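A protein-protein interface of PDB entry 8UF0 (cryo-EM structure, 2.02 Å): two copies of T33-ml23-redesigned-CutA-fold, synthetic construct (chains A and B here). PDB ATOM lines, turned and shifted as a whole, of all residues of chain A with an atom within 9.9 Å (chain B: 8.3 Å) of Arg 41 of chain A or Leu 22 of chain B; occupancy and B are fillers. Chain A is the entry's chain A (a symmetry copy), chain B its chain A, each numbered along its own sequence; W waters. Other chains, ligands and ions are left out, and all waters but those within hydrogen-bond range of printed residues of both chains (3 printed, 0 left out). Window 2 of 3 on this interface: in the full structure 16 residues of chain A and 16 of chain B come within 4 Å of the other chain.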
ATOM      1  N   LYS A  38      15.489  -5.940  17.400  1.00  0.00           N
ATOM      2  CA  LYS A  38      15.284  -5.116  16.217  1.00  0.00           C
ATOM      3  C   LYS A  38      14.056  -4.227  16.398  1.00  0.00           C
ATOM      4  O   LYS A  38      13.026  -4.679  16.895  1.00  0.00           O
ATOM      5  CB  LYS A  38      15.118  -5.981  14.967  1.00  0.00           C
ATOM      6  CG  LYS A  38      14.812  -5.185  13.724  1.00  0.00           C
ATOM      7  CD  LYS A  38      15.150  -5.917  12.460  1.00  0.00           C
ATOM      8  CE  LYS A  38      13.919  -6.520  11.841  1.00  0.00           C
ATOM      9  NZ  LYS A  38      14.218  -7.096  10.511  1.00  0.00           N
ATOM     10  N   ILE A  39      14.169  -2.963  15.988  1.00  0.00           N
ATOM     11  CA  ILE A  39      13.100  -1.976  16.107  1.00  0.00           C
ATOM     12  C   ILE A  39      12.846  -1.350  14.740  1.00  0.00           C
ATOM     13  O   ILE A  39      13.787  -0.894  14.084  1.00  0.00           O
ATOM     14  CB  ILE A  39      13.449  -0.892  17.145  1.00  0.00           C
ATOM     15  CG1 ILE A  39      13.723  -1.531  18.501  1.00  0.00           C
ATOM     16  CG2 ILE A  39      12.330   0.114  17.273  1.00  0.00           C
ATOM     17  CD1 ILE A  39      14.375  -0.624  19.477  1.00  0.00           C
ATOM     18  N   TYR A  40      11.583  -1.318  14.320  1.00  0.00           N
ATOM     19  CA  TYR A  40      11.193  -0.797  13.007  1.00  0.00           C
ATOM     20  C   TYR A  40       9.690  -0.512  13.006  1.00  0.00           C
ATOM     21  O   TYR A  40       9.013  -0.666  14.027  1.00  0.00           O
ATOM     22  CB  TYR A  40      11.595  -1.762  11.886  1.00  0.00           C
ATOM     23  CG  TYR A  40      10.766  -3.011  11.847  1.00  0.00           C
ATOM     24  CD1 TYR A  40      10.756  -3.891  12.914  1.00  0.00           C
ATOM     25  CD2 TYR A  40       9.955  -3.289  10.761  1.00  0.00           C
ATOM     26  CE1 TYR A  40       9.991  -5.019  12.890  1.00  0.00           C
ATOM     27  CE2 TYR A  40       9.180  -4.420  10.728  1.00  0.00           C
ATOM     28  CZ  TYR A  40       9.202  -5.284  11.795  1.00  0.00           C
ATOM     29  OH  TYR A  40       8.430  -6.413  11.766  1.00  0.00           O
ATOM     30  N   ARG A  41       9.163  -0.093  11.857  1.00  0.00           N
ATOM     31  CA  ARG A  41       7.775   0.351  11.737  1.00  0.00           C
ATOM     32  C   ARG A  41       6.969  -0.567  10.829  1.00  0.00           C
ATOM     33  O   ARG A  41       7.368  -0.832   9.691  1.00  0.00           O
ATOM     34  CB  ARG A  41       7.699   1.785  11.208  1.00  0.00           C
ATOM     35  CG  ARG A  41       6.290   2.350  11.193  1.00  0.00           C
ATOM     36  CD  ARG A  41       6.166   3.538  10.251  1.00  0.00           C
ATOM     37  NE  ARG A  41       7.006   4.652  10.670  1.00  0.00           N
ATOM     38  CZ  ARG A  41       8.089   5.056  10.025  1.00  0.00           C
ATOM     39  NH1 ARG A  41       8.502   4.455   8.925  1.00  0.00           N
ATOM     40  NH2 ARG A  41       8.776   6.083  10.499  1.00  0.00           N
ATOM     41  N   GLU A  42       5.823  -1.029  11.326  1.00  0.00           N
ATOM     42  CA  GLU A  42       4.883  -1.836  10.554  1.00  0.00           C
ATOM     43  C   GLU A  42       3.484  -1.250  10.681  1.00  0.00           C
ATOM     44  O   GLU A  42       2.987  -1.062  11.796  1.00  0.00           O
ATOM     45  CB  GLU A  42       4.884  -3.295  11.023  1.00  0.00           C
ATOM     46  CG  GLU A  42       4.977  -4.310   9.896  1.00  0.00           C
ATOM     47  CD  GLU A  42       4.941  -5.742  10.396  1.00  0.00           C
ATOM     48  OE1 GLU A  42       4.408  -5.980  11.499  1.00  0.00           O
ATOM     49  OE2 GLU A  42       5.456  -6.631   9.688  1.00  0.00           O
ATOM     50  N   ASN A  43       2.849  -0.979   9.537  1.00  0.00           N
ATOM     51  CA  ASN A  43       1.490  -0.434   9.485  1.00  0.00           C
ATOM     52  C   ASN A  43       1.377   0.864  10.282  1.00  0.00           C
ATOM     53  O   ASN A  43       0.446   1.065  11.062  1.00  0.00           O
ATOM     54  CB  ASN A  43       0.468  -1.461   9.974  1.00  0.00           C
ATOM     55  CG  ASN A  43       0.302  -2.613   9.011  1.00  0.00           C
ATOM     56  OD1 ASN A  43       0.245  -2.415   7.799  1.00  0.00           O
ATOM     57  ND2 ASN A  43       0.230  -3.825   9.543  1.00  0.00           N
ATOM     58  N   GLY A  44       2.353   1.743  10.089  1.00  0.00           N
ATOM     59  CA  GLY A  44       2.369   2.987  10.831  1.00  0.00           C
ATOM     60  C   GLY A  44       2.542   2.829  12.321  1.00  0.00           C
ATOM     61  O   GLY A  44       2.250   3.762  13.068  1.00  0.00           O
ATOM     62  N   GLU A  45       3.011   1.673  12.781  1.00  0.00           N
ATOM     63  CA  GLU A  45       3.237   1.444  14.197  1.00  0.00           C
ATOM     64  C   GLU A  45       4.657   0.937  14.427  1.00  0.00           C
ATOM     65  O   GLU A  45       5.224   0.240  13.585  1.00  0.00           O
ATOM     66  CB  GLU A  45       2.218   0.451  14.760  1.00  0.00           C
ATOM     67  CG  GLU A  45       2.173   0.298  16.291  1.00  0.00           C
ATOM     68  CD  GLU A  45       2.305   1.600  17.089  1.00  0.00           C
ATOM     69  OE1 GLU A  45       3.288   2.360  16.924  1.00  0.00           O
ATOM     70  OE2 GLU A  45       1.397   1.871  17.901  1.00  0.00           O
ATOM     71  N   ILE A  46       5.217   1.285  15.582  1.00  0.00           N
ATOM     72  CA  ILE A  46       6.578   0.913  15.954  1.00  0.00           C
ATOM     73  C   ILE A  46       6.531  -0.376  16.767  1.00  0.00           C
ATOM     74  O   ILE A  46       5.846  -0.440  17.790  1.00  0.00           O
ATOM     75  CB  ILE A  46       7.248   2.036  16.761  1.00  0.00           C
ATOM     76  CG1 ILE A  46       7.136   3.372  16.028  1.00  0.00           C
ATOM     77  CG2 ILE A  46       8.690   1.700  17.066  1.00  0.00           C
ATOM     78  CD1 ILE A  46       7.910   3.439  14.756  1.00  0.00           C
ATOM     79  N   LYS A  47       7.275  -1.395  16.337  1.00  0.00           N
ATOM     80  CA  LYS A  47       7.309  -2.666  17.053  1.00  0.00           C
ATOM     81  C   LYS A  47       8.741  -3.172  17.179  1.00  0.00           C
ATOM     82  O   LYS A  47       9.660  -2.679  16.525  1.00  0.00           O
ATOM     83  CB  LYS A  47       6.442  -3.713  16.359  1.00  0.00           C
ATOM     84  CG  LYS A  47       6.545  -3.686  14.859  1.00  0.00           C
ATOM     85  CD  LYS A  47       6.306  -5.064  14.302  1.00  0.00           C
ATOM     86  CE  LYS A  47       7.370  -6.036  14.757  1.00  0.00           C
ATOM     87  NZ  LYS A  47       6.850  -7.427  14.766  1.00  0.00           N
ATOM     88  N   SER A  48       8.919  -4.180  18.033  1.00  0.00           N
ATOM     89  CA  SER A  48      10.229  -4.744  18.325  1.00  0.00           C
ATOM     90  C   SER A  48      10.146  -6.266  18.395  1.00  0.00           C
ATOM     91  O   SER A  48       9.114  -6.822  18.773  1.00  0.00           O
ATOM     92  CB  SER A  48      10.787  -4.162  19.627  1.00  0.00           C
ATOM     93  OG  SER A  48      10.439  -4.952  20.739  1.00  0.00           O
ATOM     94  N   GLU A  49      11.242  -6.934  18.028  1.00  0.00           N
ATOM     95  CA  GLU A  49      11.293  -8.394  17.990  1.00  0.00           C
ATOM     96  C   GLU A  49      12.742  -8.872  18.062  1.00  0.00           C
ATOM     97  O   GLU A  49      13.682  -8.097  17.892  1.00  0.00           O
ATOM     98  CB  GLU A  49      10.612  -8.936  16.736  1.00  0.00           C
ATOM     99  CG  GLU A  49      11.274  -8.505  15.462  1.00  0.00           C
ATOM    100  CD  GLU A  49      10.465  -8.853  14.240  1.00  0.00           C
ATOM    101  OE1 GLU A  49       9.237  -9.026  14.372  1.00  0.00           O
ATOM    102  OE2 GLU A  49      11.050  -8.951  13.144  1.00  0.00           O
ATOM    103  N   LYS B  15      17.261   2.354  23.379  1.00  0.00           N
ATOM    104  CA  LYS B  15      15.952   2.249  22.741  1.00  0.00           C
ATOM    105  C   LYS B  15      15.322   3.621  22.524  1.00  0.00           C
ATOM    106  O   LYS B  15      14.671   3.854  21.502  1.00  0.00           O
ATOM    107  CB  LYS B  15      15.023   1.367  23.572  1.00  0.00           C
ATOM    108  CG  LYS B  15      15.360  -0.104  23.538  1.00  0.00           C
ATOM    109  CD  LYS B  15      14.945  -0.769  24.833  1.00  0.00           C
ATOM    110  CE  LYS B  15      14.276  -2.104  24.604  1.00  0.00           C
ATOM    111  NZ  LYS B  15      15.197  -3.090  23.988  1.00  0.00           N
ATOM    112  N   ALA B  16      15.511   4.541  23.472  1.00  0.00           N
ATOM    113  CA  ALA B  16      14.937   5.878  23.343  1.00  0.00           C
ATOM    114  C   ALA B  16      15.509   6.630  22.143  1.00  0.00           C
ATOM    115  O   ALA B  16      14.775   7.325  21.437  1.00  0.00           O
ATOM    116  CB  ALA B  16      15.155   6.669  24.631  1.00  0.00           C
ATOM    117  N   ILE B  17      16.814   6.508  21.898  1.00  0.00           N
ATOM    118  CA  ILE B  17      17.410   7.160  20.735  1.00  0.00           C
ATOM    119  C   ILE B  17      16.803   6.620  19.443  1.00  0.00           C
ATOM    120  O   ILE B  17      16.464   7.383  18.532  1.00  0.00           O
ATOM    121  CB  ILE B  17      18.942   6.994  20.752  1.00  0.00           C
ATOM    122  CG1 ILE B  17      19.571   7.882  21.820  1.00  0.00           C
ATOM    123  CG2 ILE B  17      19.544   7.316  19.400  1.00  0.00           C
ATOM    124  CD1 ILE B  17      21.046   7.666  21.987  1.00  0.00           C
ATOM    125  N   ALA B  18      16.653   5.297  19.347  1.00  0.00           N
ATOM    126  CA  ALA B  18      16.134   4.693  18.123  1.00  0.00           C
ATOM    127  C   ALA B  18      14.702   5.135  17.832  1.00  0.00           C
ATOM    128  O   ALA B  18      14.359   5.423  16.682  1.00  0.00           O
ATOM    129  CB  ALA B  18      16.214   3.172  18.210  1.00  0.00           C
ATOM    130  N   LYS B  19      13.857   5.198  18.860  1.00  0.00           N
ATOM    131  CA  LYS B  19      12.469   5.601  18.657  1.00  0.00           C
ATOM    132  C   LYS B  19      12.361   7.036  18.150  1.00  0.00           C
ATOM    133  O   LYS B  19      11.556   7.320  17.260  1.00  0.00           O
ATOM    134  CB  LYS B  19      11.679   5.418  19.949  1.00  0.00           C
ATOM    135  CG  LYS B  19      10.179   5.578  19.782  1.00  0.00           C
ATOM    136  CD  LYS B  19       9.373   5.448  21.083  1.00  0.00           C
ATOM    137  CE  LYS B  19       9.785   4.281  21.990  1.00  0.00           C
ATOM    138  NZ  LYS B  19      10.399   3.094  21.318  1.00  0.00           N
ATOM    139  N   LYS B  20      13.169   7.949  18.690  1.00  0.00           N
ATOM    140  CA  LYS B  20      13.128   9.332  18.228  1.00  0.00           C
ATOM    141  C   LYS B  20      13.515   9.445  16.759  1.00  0.00           C
ATOM    142  O   LYS B  20      12.897  10.201  16.007  1.00  0.00           O
ATOM    143  CB  LYS B  20      14.044  10.202  19.081  1.00  0.00           C
ATOM    144  CG  LYS B  20      13.409  10.725  20.334  1.00  0.00           C
ATOM    145  CD  LYS B  20      12.906  12.135  20.137  1.00  0.00           C
ATOM    146  CE  LYS B  20      12.291  12.675  21.409  1.00  0.00           C
ATOM    147  NZ  LYS B  20      13.305  12.756  22.485  1.00  0.00           N
ATOM    148  N   LEU B  21      14.533   8.705  16.329  1.00  0.00           N
ATOM    149  CA  LEU B  21      14.946   8.783  14.933  1.00  0.00           C
ATOM    150  C   LEU B  21      13.904   8.181  13.991  1.00  0.00           C
ATOM    151  O   LEU B  21      13.765   8.645  12.858  1.00  0.00           O
ATOM    152  CB  LEU B  21      16.302   8.104  14.742  1.00  0.00           C
ATOM    153  CG  LEU B  21      17.538   8.812  15.309  1.00  0.00           C
ATOM    154  CD1 LEU B  21      18.720   7.868  15.328  1.00  0.00           C
ATOM    155  CD2 LEU B  21      17.881  10.069  14.539  1.00  0.00           C
ATOM    156  N   LEU B  22      13.171   7.157  14.431  1.00  0.00           N
ATOM    157  CA  LEU B  22      12.147   6.565  13.574  1.00  0.00           C
ATOM    158  C   LEU B  22      10.940   7.483  13.418  1.00  0.00           C
ATOM    159  O   LEU B  22      10.353   7.559  12.337  1.00  0.00           O
ATOM    160  CB  LEU B  22      11.715   5.202  14.116  1.00  0.00           C
ATOM    161  CG  LEU B  22      12.594   4.001  13.761  1.00  0.00           C
ATOM    162  CD1 LEU B  22      12.319   2.837  14.694  1.00  0.00           C
ATOM    163  CD2 LEU B  22      12.434   3.579  12.304  1.00  0.00           C
ATOM    164  N   GLU B  23      10.559   8.193  14.481  1.00  0.00           N
ATOM    165  CA  GLU B  23       9.403   9.083  14.405  1.00  0.00           C
ATOM    166  C   GLU B  23       9.636  10.260  13.467  1.00  0.00           C
ATOM    167  O   GLU B  23       8.684  10.778  12.885  1.00  0.00           O
ATOM    168  CB  GLU B  23       9.035   9.589  15.794  1.00  0.00           C
ATOM    169  CG  GLU B  23       8.240   8.596  16.593  1.00  0.00           C
ATOM    170  CD  GLU B  23       8.307   8.853  18.080  1.00  0.00           C
ATOM    171  OE1 GLU B  23       9.155   9.656  18.513  1.00  0.00           O
ATOM    172  OE2 GLU B  23       7.507   8.251  18.820  1.00  0.00           O
ATOM    173  N   ASN B  24      10.877  10.692  13.303  1.00  0.00           N
ATOM    174  CA  ASN B  24      11.211  11.782  12.403  1.00  0.00           C
ATOM    175  C   ASN B  24      11.506  11.304  10.989  1.00  0.00           C
ATOM    176  O   ASN B  24      11.869  12.120  10.141  1.00  0.00           O
ATOM    177  CB  ASN B  24      12.415  12.546  12.950  1.00  0.00           C
ATOM    178  CG  ASN B  24      12.026  13.587  13.975  1.00  0.00           C
ATOM    179  OD1 ASN B  24      11.928  13.296  15.164  1.00  0.00           O
ATOM    180  ND2 ASN B  24      11.815  14.807  13.523  1.00  0.00           N
ATOM    181  N   ARG B  25      11.383  10.001  10.732  1.00  0.00           N
ATOM    182  CA  ARG B  25      11.611   9.396   9.419  1.00  0.00           C
ATOM    183  C   ARG B  25      13.033   9.631   8.905  1.00  0.00           C
ATOM    184  O   ARG B  25      13.254   9.823   7.712  1.00  0.00           O
ATOM    185  CB  ARG B  25      10.572   9.880   8.401  1.00  0.00           C
ATOM    186  CG  ARG B  25       9.217   9.194   8.537  1.00  0.00           C
ATOM    187  CD  ARG B  25       8.212   9.692   7.518  1.00  0.00           C
ATOM    188  NE  ARG B  25       8.390   9.051   6.220  1.00  0.00           N
ATOM    189  CZ  ARG B  25       7.933   7.847   5.906  1.00  0.00           C
ATOM    190  NH1 ARG B  25       7.223   7.132   6.763  1.00  0.00           N
ATOM    191  NH2 ARG B  25       8.198   7.348   4.704  1.00  0.00           N
ATOM    192  N   LEU B  26      14.015   9.587   9.801  1.00  0.00           N
ATOM    193  CA  LEU B  26      15.404   9.742   9.396  1.00  0.00           C
ATOM    194  C   LEU B  26      16.141   8.418   9.190  1.00  0.00           C
ATOM    195  O   LEU B  26      17.185   8.415   8.540  1.00  0.00           O
ATOM    196  CB  LEU B  26      16.162  10.605  10.414  1.00  0.00           C
ATOM    197  CG  LEU B  26      15.751  12.084  10.496  1.00  0.00           C
ATOM    198  CD1 LEU B  26      16.438  12.810  11.640  1.00  0.00           C
ATOM    199  CD2 LEU B  26      16.003  12.807   9.188  1.00  0.00           C
ATOM    200  N   ILE B  27      15.626   7.301   9.708  1.00  0.00           N
ATOM    201  CA  ILE B  27      16.217   5.976   9.528  1.00  0.00           C
ATOM    202  C   ILE B  27      15.105   4.981   9.219  1.00  0.00           C
ATOM    203  O   ILE B  27      13.926   5.257   9.413  1.00  0.00           O
ATOM    204  CB  ILE B  27      17.013   5.494  10.765  1.00  0.00           C
ATOM    205  CG1 ILE B  27      16.074   5.318  11.962  1.00  0.00           C
ATOM    206  CG2 ILE B  27      18.171   6.425  11.082  1.00  0.00           C
ATOM    207  CD1 ILE B  27      16.642   4.523  13.075  1.00  0.00           C
ATOM    208  N   ALA B  28      15.501   3.793   8.768  1.00  0.00           N
ATOM    209  CA  ALA B  28      14.564   2.722   8.453  1.00  0.00           C
ATOM    210  C   ALA B  28      14.457   1.644   9.532  1.00  0.00           C
ATOM    211  O   ALA B  28      13.363   1.131   9.750  1.00  0.00           O
ATOM    212  CB  ALA B  28      14.932   2.076   7.117  1.00  0.00           C
ATOM    213  N   GLU B  29      15.548   1.274  10.209  1.00  0.00           N
ATOM    214  CA  GLU B  29      15.494   0.293  11.296  1.00  0.00           C
ATOM    215  C   GLU B  29      16.770   0.369  12.135  1.00  0.00           C
ATOM    216  O   GLU B  29      17.756   0.986  11.736  1.00  0.00           O
ATOM    217  CB  GLU B  29      15.272  -1.135  10.769  1.00  0.00           C
ATOM    218  CG  GLU B  29      16.284  -1.621   9.760  1.00  0.00           C
ATOM    219  CD  GLU B  29      15.983  -3.028   9.246  1.00  0.00           C
ATOM    220  OE1 GLU B  29      14.928  -3.592   9.602  1.00  0.00           O
ATOM    221  OE2 GLU B  29      16.797  -3.573   8.473  1.00  0.00           O
ATOM    222  N   ALA B  30      16.739  -0.286  13.301  1.00  0.00           N
ATOM    223  CA  ALA B  30      17.848  -0.285  14.256  1.00  0.00           C
ATOM    224  C   ALA B  30      18.012  -1.648  14.934  1.00  0.00           C
ATOM    225  O   ALA B  30      17.032  -2.344  15.195  1.00  0.00           O
ATOM    226  CB  ALA B  30      17.649   0.796  15.325  1.00  0.00           C
ATOM    227  N   LEU B  56      22.440   1.603  13.162  1.00  0.00           N
ATOM    228  CA  LEU B  56      21.332   2.218  12.435  1.00  0.00           C
ATOM    229  C   LEU B  56      21.567   2.178  10.928  1.00  0.00           C
ATOM    230  O   LEU B  56      22.685   2.399  10.460  1.00  0.00           O
ATOM    231  CB  LEU B  56      21.111   3.671  12.886  1.00  0.00           C
ATOM    232  CG  LEU B  56      21.240   3.960  14.385  1.00  0.00           C
ATOM    233  CD1 LEU B  56      21.639   5.391  14.625  1.00  0.00           C
ATOM    234  CD2 LEU B  56      19.971   3.627  15.142  1.00  0.00           C
ATOM    235  N   TYR B  57      20.503   1.922  10.168  1.00  0.00           N
ATOM    236  CA  TYR B  57      20.570   1.738   8.720  1.00  0.00           C
ATOM    237  C   TYR B  57      19.759   2.817   8.011  1.00  0.00           C
ATOM    238  O   TYR B  57      18.580   3.006   8.315  1.00  0.00           O
ATOM    239  CB  TYR B  57      20.056   0.343   8.330  1.00  0.00           C
ATOM    240  CG  TYR B  57      20.803  -0.791   8.993  1.00  0.00           C
ATOM    241  CD1 TYR B  57      20.482  -1.204  10.280  1.00  0.00           C
ATOM    242  CD2 TYR B  57      21.846  -1.433   8.343  1.00  0.00           C
ATOM    243  CE1 TYR B  57      21.169  -2.219  10.893  1.00  0.00           C
ATOM    244  CE2 TYR B  57      22.540  -2.456   8.949  1.00  0.00           C
ATOM    245  CZ  TYR B  57      22.194  -2.847  10.222  1.00  0.00           C
ATOM    246  OH  TYR B  57      22.878  -3.862  10.830  1.00  0.00           O
ATOM    247  N   TRP B  96      13.519  -1.085  -0.528  1.00  0.00           N
ATOM    248  CA  TRP B  96      12.715  -1.032   0.692  1.00  0.00           C
ATOM    249  C   TRP B  96      13.160   0.107   1.609  1.00  0.00           C
ATOM    250  O   TRP B  96      12.324   0.794   2.200  1.00  0.00           O
ATOM    251  CB  TRP B  96      12.768  -2.375   1.427  1.00  0.00           C
ATOM    252  CG  TRP B  96      11.977  -2.389   2.703  1.00  0.00           C
ATOM    253  CD1 TRP B  96      10.639  -2.569   2.831  1.00  0.00           C
ATOM    254  CD2 TRP B  96      12.480  -2.189   4.026  1.00  0.00           C
ATOM    255  NE1 TRP B  96      10.272  -2.501   4.144  1.00  0.00           N
ATOM    256  CE2 TRP B  96      11.386  -2.268   4.902  1.00  0.00           C
ATOM    257  CE3 TRP B  96      13.751  -1.955   4.554  1.00  0.00           C
ATOM    258  CZ2 TRP B  96      11.521  -2.123   6.280  1.00  0.00           C
ATOM    259  CZ3 TRP B  96      13.883  -1.814   5.921  1.00  0.00           C
ATOM    260  CH2 TRP B  96      12.775  -1.898   6.769  1.00  0.00           C
ATOM    261  N   VAL B  97      14.471   0.329   1.728  1.00  0.00           N
ATOM    262  CA  VAL B  97      14.978   1.394   2.593  1.00  0.00           C
ATOM    263  C   VAL B  97      14.513   2.761   2.098  1.00  0.00           C
ATOM    264  O   VAL B  97      14.079   3.603   2.888  1.00  0.00           O
ATOM    265  CB  VAL B  97      16.516   1.317   2.699  1.00  0.00           C
ATOM    266  CG1 VAL B  97      17.095   2.624   3.229  1.00  0.00           C
ATOM    267  CG2 VAL B  97      16.936   0.159   3.581  1.00  0.00           C
ATOM    268  N   PHE B  99      11.838   3.361   0.269  1.00  0.00           N
ATOM    269  CA  PHE B  99      10.393   3.425   0.465  1.00  0.00           C
ATOM    270  C   PHE B  99      10.027   3.813   1.895  1.00  0.00           C
ATOM    271  O   PHE B  99       9.021   4.493   2.111  1.00  0.00           O
ATOM    272  CB  PHE B  99       9.779   2.075   0.090  1.00  0.00           C
ATOM    273  CG  PHE B  99       8.289   1.983   0.269  1.00  0.00           C
ATOM    274  CD1 PHE B  99       7.432   2.329  -0.755  1.00  0.00           C
ATOM    275  CD2 PHE B  99       7.747   1.495   1.441  1.00  0.00           C
ATOM    276  CE1 PHE B  99       6.068   2.219  -0.604  1.00  0.00           C
ATOM    277  CE2 PHE B  99       6.381   1.387   1.597  1.00  0.00           C
ATOM    278  CZ  PHE B  99       5.542   1.749   0.575  1.00  0.00           C
ATOM    279  N   GLU B 100      10.820   3.389   2.880  1.00  0.00           N
ATOM    280  CA  GLU B 100      10.484   3.628   4.280  1.00  0.00           C
ATOM    281  C   GLU B 100      10.885   5.011   4.777  1.00  0.00           C
ATOM    282  O   GLU B 100      10.335   5.468   5.779  1.00  0.00           O
ATOM    283  CB  GLU B 100      11.142   2.575   5.171  1.00  0.00           C
ATOM    284  CG  GLU B 100      10.464   1.228   5.142  1.00  0.00           C
ATOM    285  CD  GLU B 100       9.030   1.290   5.598  1.00  0.00           C
ATOM    286  OE1 GLU B 100       8.749   1.972   6.599  1.00  0.00           O
ATOM    287  OE2 GLU B 100       8.175   0.653   4.961  1.00  0.00           O
ATOM    288  N   THR B 101      11.825   5.676   4.123  1.00  0.00           N
ATOM    289  CA  THR B 101      12.254   6.994   4.564  1.00  0.00           C
ATOM    290  C   THR B 101      11.818   8.069   3.575  1.00  0.00           C
ATOM    291  O   THR B 101      12.616   8.899   3.149  1.00  0.00           O
ATOM    292  CB  THR B 101      13.787   7.072   4.757  1.00  0.00           C
ATOM    293  OG1 THR B 101      14.455   6.683   3.552  1.00  0.00           O
ATOM    294  CG2 THR B 101      14.239   6.177   5.904  1.00  0.00           C
ATOM    295  OXT THR B 101      10.657   8.135   3.176  1.00  0.00           O
HETATM  296  O   HOH W   1      10.574   0.839   9.771  1.00  0.00           O
HETATM  297  O   HOH W   2      14.863  -5.996   7.610  1.00  0.00           O
HETATM  298  O   HOH W   3      11.098   5.761   8.838  1.00  0.00           O
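Of chain B, only Leu 22, Arg 25 and Glu 100 come within 4 Å of Arg 41 of chain A.
Of chain A, only Ile 39 (3.8 Å) and Arg 41 (2.8 Å) come within 4 Å of Leu 22 of chain B.
Leu 21 of chain B touches none of the printed residues of chain A.
Printed residues of chain A within 4 Å of Arg 25 of chain B: Arg 41 (3.7 Å).
Of the printed residues of chain A, Glu 29 of chain B touches Lys 38 (3.7 Å), Ile 39 (3.5 Å) and Tyr 40 (3.9 Å).
Ala 16 of chain B touches none of the printed residues of chain A.
The nearest printed residue of chain A that does not touch Arg 25 of chain B is Gly 44 of chain A (7.6 Å).
No position is printed for both chains.
Of the 23 printed residues of chain B, 5 touch a printed residue of chain A.
Of the 12 printed residues of chain A, 4 touch a printed residue of chain B.
Hydrophobic or aromatic side chains of chain A within 4 Å of the printed part of chain B: Ile 39 and Tyr 40.
Among the printed residues, 9 pairs touch across the chains.
Water W1 lies within hydrogen-bond range of the backbone NH (N) of Arg 41 of chain A (2.7 Å) and the backbone carbonyl oxygen (O) of Ala 28 of chain B (2.8 Å).
Water W3 lies within hydrogen-bond range of NH2 of Arg 41 of chain A, O of Ile 27 of chain B and O of Glu 100 of chain B.
Water W2 lies within hydrogen-bond range of the side-chain carboxylate of Glu 29 of chain B (3.1 Å) and the side-chain amino group of Lys 38 of chain A (3.2 Å).
Among the printed residues, pairs that only touch across the chains: Lys 38 of chain A with Ala 30 of chain B, Ile 39 of chain A with Leu 22 of chain B, Ile 39 of chain A with Glu 29 of chain B, Tyr 40 of chain A with Glu 29 of chain B and Arg 41 of chain A with Arg 25 of chain B.
The guanidinium group (NH2) of Arg 25 of chain B is in hydrogen-bond range of the backbone carbonyl oxygen (O) of Glu 100 of chain B (3.0 Å).
The guanidinium group of Arg 25 of chain B lies within salt-bridge range of the chain-end carboxylate of Thr 101 of chain B, 3.0 Å away.
N of Tyr 57 of chain B is in hydrogen-bond range of O of Glu 29 of chain B (3.3 Å).
O of Glu 49 of chain A is in hydrogen-bond range of N of Lys 38 of chain A (2.9 Å).
The backbone carbonyl oxygen of Tyr 40 of chain A sits at hydrogen-bond distance from the backbone NH of Lys 47 of chain A, at 3.0 Å.
O of Leu 22 of chain B lies within hydrogen-bond range of NH2 of Arg 41 of chain A (2.8 Å).
OE1 of Glu 29 of chain B lies within salt-bridge range of NZ of Lys 38 of chain A (3.7 Å).
The backbone carbonyl oxygen (O) of Ala 30 of chain B is in hydrogen-bond range of the backbone NH (N) of Ile 39 of chain A.
The side-chain carboxylate (OE1) of Glu 100 of chain B lies within salt-bridge range of the guanidinium group (NH1) of Arg 41 of chain A.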
